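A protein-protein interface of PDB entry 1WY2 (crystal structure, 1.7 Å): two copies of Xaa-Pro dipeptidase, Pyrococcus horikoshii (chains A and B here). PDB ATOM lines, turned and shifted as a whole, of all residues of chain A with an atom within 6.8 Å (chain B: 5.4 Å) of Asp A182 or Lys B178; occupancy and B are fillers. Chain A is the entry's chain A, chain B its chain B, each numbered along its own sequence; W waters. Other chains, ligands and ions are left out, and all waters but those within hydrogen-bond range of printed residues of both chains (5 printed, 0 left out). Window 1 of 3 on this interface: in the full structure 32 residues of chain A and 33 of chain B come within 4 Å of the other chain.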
ATOM      1  N   ARG A 161       1.702  22.893 -30.657  1.00  0.00           N
ATOM      2  CA  ARG A 161       0.414  22.758 -29.985  1.00  0.00           C
ATOM      3  C   ARG A 161       0.527  22.187 -28.577  1.00  0.00           C
ATOM      4  O   ARG A 161      -0.250  22.549 -27.694  1.00  0.00           O
ATOM      5  CB  ARG A 161      -0.516  21.873 -30.813  1.00  0.00           C
ATOM      6  CG  ARG A 161      -1.868  21.619 -30.164  1.00  0.00           C
ATOM      7  CD  ARG A 161      -2.989  22.033 -31.086  1.00  0.00           C
ATOM      8  NE  ARG A 161      -2.784  21.521 -32.436  1.00  0.00           N
ATOM      9  CZ  ARG A 161      -3.372  22.018 -33.517  1.00  0.00           C
ATOM     10  NH1 ARG A 161      -4.205  23.042 -33.407  1.00  0.00           N
ATOM     11  NH2 ARG A 161      -3.116  21.498 -34.709  1.00  0.00           N
ATOM     12  N   GLU A 168      -1.401  26.848 -21.365  1.00  0.00           N
ATOM     13  CA  GLU A 168      -2.786  27.257 -21.184  1.00  0.00           C
ATOM     14  C   GLU A 168      -3.317  26.581 -19.925  1.00  0.00           C
ATOM     15  O   GLU A 168      -4.146  27.143 -19.211  1.00  0.00           O
ATOM     16  CB  GLU A 168      -3.617  26.898 -22.415  1.00  0.00           C
ATOM     17  CG  GLU A 168      -3.218  27.742 -23.633  1.00  0.00           C
ATOM     18  CD  GLU A 168      -4.006  27.421 -24.884  1.00  0.00           C
ATOM     19  OE1 GLU A 168      -4.550  26.300 -24.975  1.00  0.00           O
ATOM     20  OE2 GLU A 168      -4.062  28.288 -25.788  1.00  0.00           O
ATOM     21  N   PRO A 179      -7.514  31.213 -21.800  1.00  0.00           N
ATOM     22  CA  PRO A 179      -6.578  32.079 -22.527  1.00  0.00           C
ATOM     23  C   PRO A 179      -7.337  33.277 -23.094  1.00  0.00           C
ATOM     24  O   PRO A 179      -8.512  33.160 -23.437  1.00  0.00           O
ATOM     25  CB  PRO A 179      -6.042  31.164 -23.632  1.00  0.00           C
ATOM     26  CG  PRO A 179      -6.186  29.786 -23.047  1.00  0.00           C
ATOM     27  CD  PRO A 179      -7.537  29.861 -22.384  1.00  0.00           C
ATOM     28  N   ALA A 180      -6.671  34.423 -23.198  1.00  0.00           N
ATOM     29  CA  ALA A 180      -7.315  35.625 -23.726  1.00  0.00           C
ATOM     30  C   ALA A 180      -7.593  35.485 -25.221  1.00  0.00           C
ATOM     31  O   ALA A 180      -8.463  36.164 -25.774  1.00  0.00           O
ATOM     32  CB  ALA A 180      -6.433  36.846 -23.468  1.00  0.00           C
ATOM     33  N   PHE A 181      -6.840  34.599 -25.863  1.00  0.00           N
ATOM     34  CA  PHE A 181      -6.977  34.338 -27.290  1.00  0.00           C
ATOM     35  C   PHE A 181      -6.179  33.078 -27.609  1.00  0.00           C
ATOM     36  O   PHE A 181      -5.406  32.613 -26.778  1.00  0.00           O
ATOM     37  CB  PHE A 181      -6.456  35.535 -28.093  1.00  0.00           C
ATOM     38  CG  PHE A 181      -5.059  35.956 -27.726  1.00  0.00           C
ATOM     39  CD1 PHE A 181      -3.957  35.342 -28.311  1.00  0.00           C
ATOM     40  CD2 PHE A 181      -4.846  36.966 -26.792  1.00  0.00           C
ATOM     41  CE1 PHE A 181      -2.664  35.728 -27.974  1.00  0.00           C
ATOM     42  CE2 PHE A 181      -3.552  37.362 -26.444  1.00  0.00           C
ATOM     43  CZ  PHE A 181      -2.460  36.744 -27.037  1.00  0.00           C
ATOM     44  N   ASP A 182      -6.376  32.521 -28.802  1.00  0.00           N
ATOM     45  CA  ASP A 182      -5.667  31.307 -29.205  1.00  0.00           C
ATOM     46  C   ASP A 182      -4.153  31.511 -29.150  1.00  0.00           C
ATOM     47  O   ASP A 182      -3.597  32.326 -29.886  1.00  0.00           O
ATOM     48  CB  ASP A 182      -6.097  30.893 -30.617  1.00  0.00           C
ATOM     49  CG  ASP A 182      -7.498  30.304 -30.652  1.00  0.00           C
ATOM     50  OD1 ASP A 182      -8.422  30.913 -30.073  1.00  0.00           O
ATOM     51  OD2 ASP A 182      -7.676  29.230 -31.266  1.00  0.00           O
ATOM     52  N   THR A 183      -3.494  30.752 -28.282  1.00  0.00           N
ATOM     53  CA  THR A 183      -2.052  30.864 -28.091  1.00  0.00           C
ATOM     54  C   THR A 183      -1.234  30.652 -29.350  1.00  0.00           C
ATOM     55  O   THR A 183      -1.422  29.677 -30.082  1.00  0.00           O
ATOM     56  CB  THR A 183      -1.560  29.878 -27.016  1.00  0.00           C
ATOM     57  OG1 THR A 183      -2.173  30.206 -25.764  1.00  0.00           O
ATOM     58  CG2 THR A 183      -0.044  29.955 -26.865  1.00  0.00           C
ATOM     59  N   ILE A 184      -0.313  31.581 -29.582  1.00  0.00           N
ATOM     60  CA  ILE A 184       0.566  31.525 -30.734  1.00  0.00           C
ATOM     61  C   ILE A 184       1.942  31.017 -30.329  1.00  0.00           C
ATOM     62  O   ILE A 184       2.601  31.611 -29.483  1.00  0.00           O
ATOM     63  CB  ILE A 184       0.718  32.927 -31.372  1.00  0.00           C
ATOM     64  CG1 ILE A 184      -0.586  33.315 -32.069  1.00  0.00           C
ATOM     65  CG2 ILE A 184       1.892  32.944 -32.356  1.00  0.00           C
ATOM     66  CD1 ILE A 184      -0.672  34.778 -32.437  1.00  0.00           C
ATOM     67  N   ILE A 185       2.337  29.887 -30.907  1.00  0.00           N
ATOM     68  CA  ILE A 185       3.657  29.304 -30.696  1.00  0.00           C
ATOM     69  C   ILE A 185       4.047  29.036 -32.144  1.00  0.00           C
ATOM     70  O   ILE A 185       3.684  28.004 -32.709  1.00  0.00           O
ATOM     71  CB  ILE A 185       3.622  27.959 -29.931  1.00  0.00           C
ATOM     72  CG1 ILE A 185       2.980  28.135 -28.549  1.00  0.00           C
ATOM     73  CG2 ILE A 185       5.047  27.425 -29.780  1.00  0.00           C
ATOM     74  CD1 ILE A 185       3.745  29.051 -27.612  1.00  0.00           C
ATOM     75  N   GLY A 196       0.367  33.092 -36.330  1.00  0.00           N
ATOM     76  CA  GLY A 196       0.604  31.666 -36.474  1.00  0.00           C
ATOM     77  C   GLY A 196       0.253  30.859 -35.238  1.00  0.00           C
ATOM     78  O   GLY A 196       1.133  30.433 -34.493  1.00  0.00           O
ATOM     79  N   VAL A 197      -1.041  30.646 -35.018  1.00  0.00           N
ATOM     80  CA  VAL A 197      -1.503  29.879 -33.868  1.00  0.00           C
ATOM     81  C   VAL A 197      -0.765  28.540 -33.800  1.00  0.00           C
ATOM     82  O   VAL A 197      -0.480  27.925 -34.831  1.00  0.00           O
ATOM     83  CB  VAL A 197      -3.027  29.645 -33.951  1.00  0.00           C
ATOM     84  CG1 VAL A 197      -3.490  28.744 -32.812  1.00  0.00           C
ATOM     85  CG2 VAL A 197      -3.749  30.984 -33.880  1.00  0.00           C
ATOM     86  N   ALA A 198      -0.444  28.102 -32.586  1.00  0.00           N
ATOM     87  CA  ALA A 198       0.279  26.847 -32.379  1.00  0.00           C
ATOM     88  C   ALA A 198      -0.287  25.727 -33.249  1.00  0.00           C
ATOM     89  O   ALA A 198      -1.500  25.518 -33.286  1.00  0.00           O
ATOM     90  CB  ALA A 198       0.220  26.452 -30.908  1.00  0.00           C
ATOM     91  N   ASP A 212       3.147  34.294 -28.376  1.00  0.00           N
ATOM     92  CA  ASP A 212       2.178  35.364 -28.140  1.00  0.00           C
ATOM     93  C   ASP A 212       0.990  34.730 -27.419  1.00  0.00           C
ATOM     94  O   ASP A 212       0.312  33.857 -27.963  1.00  0.00           O
ATOM     95  CB  ASP A 212       1.735  35.965 -29.483  1.00  0.00           C
ATOM     96  CG  ASP A 212       0.988  37.283 -29.336  1.00  0.00           C
ATOM     97  OD1 ASP A 212       0.442  37.570 -28.248  1.00  0.00           O
ATOM     98  OD2 ASP A 212       0.931  38.032 -30.335  1.00  0.00           O
ATOM     99  N   LEU A 213       0.743  35.164 -26.189  1.00  0.00           N
ATOM    100  CA  LEU A 213      -0.343  34.601 -25.403  1.00  0.00           C
ATOM    101  C   LEU A 213      -0.900  35.630 -24.436  1.00  0.00           C
ATOM    102  O   LEU A 213      -0.369  36.735 -24.301  1.00  0.00           O
ATOM    103  CB  LEU A 213       0.168  33.366 -24.636  1.00  0.00           C
ATOM    104  CG  LEU A 213       1.355  33.558 -23.681  1.00  0.00           C
ATOM    105  CD1 LEU A 213       0.867  34.112 -22.351  1.00  0.00           C
ATOM    106  CD2 LEU A 213       2.064  32.222 -23.455  1.00  0.00           C
ATOM    107  N   LYS B 172      -6.415  19.121 -26.327  1.00  0.00           N
ATOM    108  CA  LYS B 172      -5.422  19.807 -27.147  1.00  0.00           C
ATOM    109  C   LYS B 172      -4.241  18.884 -27.449  1.00  0.00           C
ATOM    110  O   LYS B 172      -3.661  18.939 -28.533  1.00  0.00           O
ATOM    111  CB  LYS B 172      -4.948  21.081 -26.437  1.00  0.00           C
ATOM    112  CG  LYS B 172      -4.238  22.069 -27.346  1.00  0.00           C
ATOM    113  CD  LYS B 172      -4.559  23.506 -26.942  1.00  0.00           C
ATOM    114  CE  LYS B 172      -4.013  24.503 -27.944  1.00  0.00           C
ATOM    115  NZ  LYS B 172      -4.499  25.885 -27.666  1.00  0.00           N
ATOM    116  N   ALA B 176      -6.876  18.866 -30.800  1.00  0.00           N
ATOM    117  CA  ALA B 176      -7.894  19.907 -30.842  1.00  0.00           C
ATOM    118  C   ALA B 176      -7.238  21.279 -30.773  1.00  0.00           C
ATOM    119  O   ALA B 176      -6.189  21.445 -30.148  1.00  0.00           O
ATOM    120  CB  ALA B 176      -8.871  19.740 -29.682  1.00  0.00           C
ATOM    121  N   GLU B 177      -7.861  22.256 -31.423  1.00  0.00           N
ATOM    122  CA  GLU B 177      -7.363  23.627 -31.423  1.00  0.00           C
ATOM    123  C   GLU B 177      -7.628  24.233 -30.051  1.00  0.00           C
ATOM    124  O   GLU B 177      -6.822  25.009 -29.532  1.00  0.00           O
ATOM    125  CB  GLU B 177      -8.101  24.463 -32.472  1.00  0.00           C
ATOM    126  CG  GLU B 177      -7.906  24.024 -33.911  1.00  0.00           C
ATOM    127  CD  GLU B 177      -8.822  24.776 -34.864  1.00  0.00           C
ATOM    128  OE1 GLU B 177      -8.874  26.024 -34.779  1.00  0.00           O
ATOM    129  OE2 GLU B 177      -9.490  24.124 -35.694  1.00  0.00           O
ATOM    130  N   LYS B 178      -8.772  23.867 -29.480  1.00  0.00           N
ATOM    131  CA  LYS B 178      -9.211  24.357 -28.179  1.00  0.00           C
ATOM    132  C   LYS B 178     -10.589  23.754 -27.907  1.00  0.00           C
ATOM    133  O   LYS B 178     -11.121  23.024 -28.743  1.00  0.00           O
ATOM    134  CB  LYS B 178      -9.315  25.885 -28.209  1.00  0.00           C
ATOM    135  CG  LYS B 178     -10.263  26.420 -29.277  1.00  0.00           C
ATOM    136  CD  LYS B 178     -10.264  27.945 -29.285  1.00  0.00           C
ATOM    137  CE  LYS B 178     -11.165  28.494 -30.371  1.00  0.00           C
ATOM    138  NZ  LYS B 178     -11.107  29.982 -30.420  1.00  0.00           N
ATOM    139  N   PRO B 179     -11.175  24.024 -26.728  1.00  0.00           N
ATOM    140  CA  PRO B 179     -12.502  23.458 -26.458  1.00  0.00           C
ATOM    141  C   PRO B 179     -13.509  24.130 -27.388  1.00  0.00           C
ATOM    142  O   PRO B 179     -13.334  25.295 -27.755  1.00  0.00           O
ATOM    143  CB  PRO B 179     -12.755  23.832 -24.994  1.00  0.00           C
ATOM    144  CG  PRO B 179     -11.379  23.974 -24.424  1.00  0.00           C
ATOM    145  CD  PRO B 179     -10.637  24.687 -25.528  1.00  0.00           C
ATOM    146  N   ALA B 180     -14.559  23.407 -27.762  1.00  0.00           N
ATOM    147  CA  ALA B 180     -15.576  23.957 -28.651  1.00  0.00           C
ATOM    148  C   ALA B 180     -16.345  25.070 -27.946  1.00  0.00           C
ATOM    149  O   ALA B 180     -16.884  25.972 -28.584  1.00  0.00           O
ATOM    150  CB  ALA B 180     -16.536  22.853 -29.092  1.00  0.00           C
ATOM    151  N   GLY B 214     -16.759  19.738 -25.551  1.00  0.00           N
ATOM    152  CA  GLY B 214     -16.636  19.492 -26.972  1.00  0.00           C
ATOM    153  C   GLY B 214     -15.272  19.930 -27.455  1.00  0.00           C
ATOM    154  O   GLY B 214     -14.596  20.729 -26.800  1.00  0.00           O
ATOM    155  N   ALA B 215     -14.856  19.407 -28.601  1.00  0.00           N
ATOM    156  CA  ALA B 215     -13.569  19.785 -29.146  1.00  0.00           C
ATOM    157  C   ALA B 215     -13.724  20.478 -30.485  1.00  0.00           C
ATOM    158  O   ALA B 215     -14.604  20.135 -31.278  1.00  0.00           O
ATOM    159  CB  ALA B 215     -12.679  18.549 -29.310  1.00  0.00           C
ATOM    160  N   LEU B 216     -12.882  21.479 -30.713  1.00  0.00           N
ATOM    161  CA  LEU B 216     -12.854  22.175 -31.993  1.00  0.00           C
ATOM    162  C   LEU B 216     -11.645  21.511 -32.647  1.00  0.00           C
ATOM    163  O   LEU B 216     -10.516  21.649 -32.170  1.00  0.00           O
ATOM    164  CB  LEU B 216     -12.610  23.676 -31.817  1.00  0.00           C
ATOM    165  CG  LEU B 216     -12.402  24.431 -33.137  1.00  0.00           C
ATOM    166  CD1 LEU B 216     -13.612  24.229 -34.042  1.00  0.00           C
ATOM    167  CD2 LEU B 216     -12.183  25.914 -32.864  1.00  0.00           C
HETATM  168  O   HOH W   1      -7.003  27.862 -33.288  1.00  0.00           O
HETATM  169  O   HOH W   2      -5.651  27.008 -31.206  1.00  0.00           O
HETATM  170  O   HOH W   3      -3.087  27.394 -29.536  1.00  0.00           O
HETATM  171  O   HOH W   4     -10.921  32.993 -28.860  1.00  0.00           O
HETATM  172  O   HOH W   5      -6.059  28.601 -27.657  1.00  0.00           O
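The side-chain carboxylate (OE1) of Glu A168 is in salt-bridge range of the side-chain amino group (NZ) of Lys B172 (2.7 Å).
The side-chain carboxylate (OD1) of Asp A182 lies within salt-bridge range of the side-chain amino group (NZ) of Lys B178.
The side-chain carboxylate of Glu A168 lies within hydrogen-bond range of the side-chain hydroxyl of Thr A183 (2.7 Å).
O of Leu B216 lies within hydrogen-bond range of N of Glu B177, 2.8 Å away.
The side-chain amino group of Lys B172 is in hydrogen-bond range of the backbone carbonyl oxygen of Glu B177, at 3.1 Å.
The backbone carbonyl oxygen (O) of Lys B178 sits at hydrogen-bond distance from the backbone NH (N) of Leu B216.
Among the printed residues, merely in contact across the chains: Arg A161 with Lys B172, Arg A161 with Ala B176 and Arg A161 with Glu B177.
Asp A182 touches just one residue of chain B: Lys B178.
Printed residues of chain B within 4 Å of Glu A168: Lys B172 (2.7 Å).
Of the printed residues of chain A, Lys B172 touches Arg A161 (3.6 Å) and Glu A168 (2.7 Å).
Printed residues of chain A within 4 Å of Ala B176: Arg A161 (3.4 Å).
Of the printed residues of chain A, Glu B177 touches Arg A161.
Of the printed residues of chain B, Arg A161 touches Lys B172 (3.6 Å), Ala B176 (3.4 Å) and Glu B177 (3.8 Å).
Pro A179 touches none of the printed residues of chain B.
The nearest residue of chain B that does not touch Asp A182 is Glu B177 (4.6 Å).
Of the 14 printed residues of chain A, 3 touch a printed residue of chain B.
2 positions are printed for both chains.
Of the 5 pairs that touch across the chains among the printed residues, none has its exchanged pair printed and touching as well.
Water W1 lies within hydrogen-bond range of OD2 of Asp A182 (2.5 Å) and OE1 of Glu B177 (3.0 Å).
Water W5 lies within hydrogen-bond range of OE2 of Glu A168 (2.8 Å), NZ of Lys B172 (3.1 Å) and N of Thr A183 (3.4 Å).
Water W3 lies within hydrogen-bond range of the side-chain amino group of Lys B172 and the backbone carbonyl oxygen of Thr A183.
Water W2 bridges the backbone carbonyl oxygen (O) of Glu B177 (2.9 Å) and the side-chain carboxylate (OD2) of Asp A182 (3.0 Å).
Water W4 lies within hydrogen-bond range of NZ of Lys B178 and OD1 of Asp A182.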
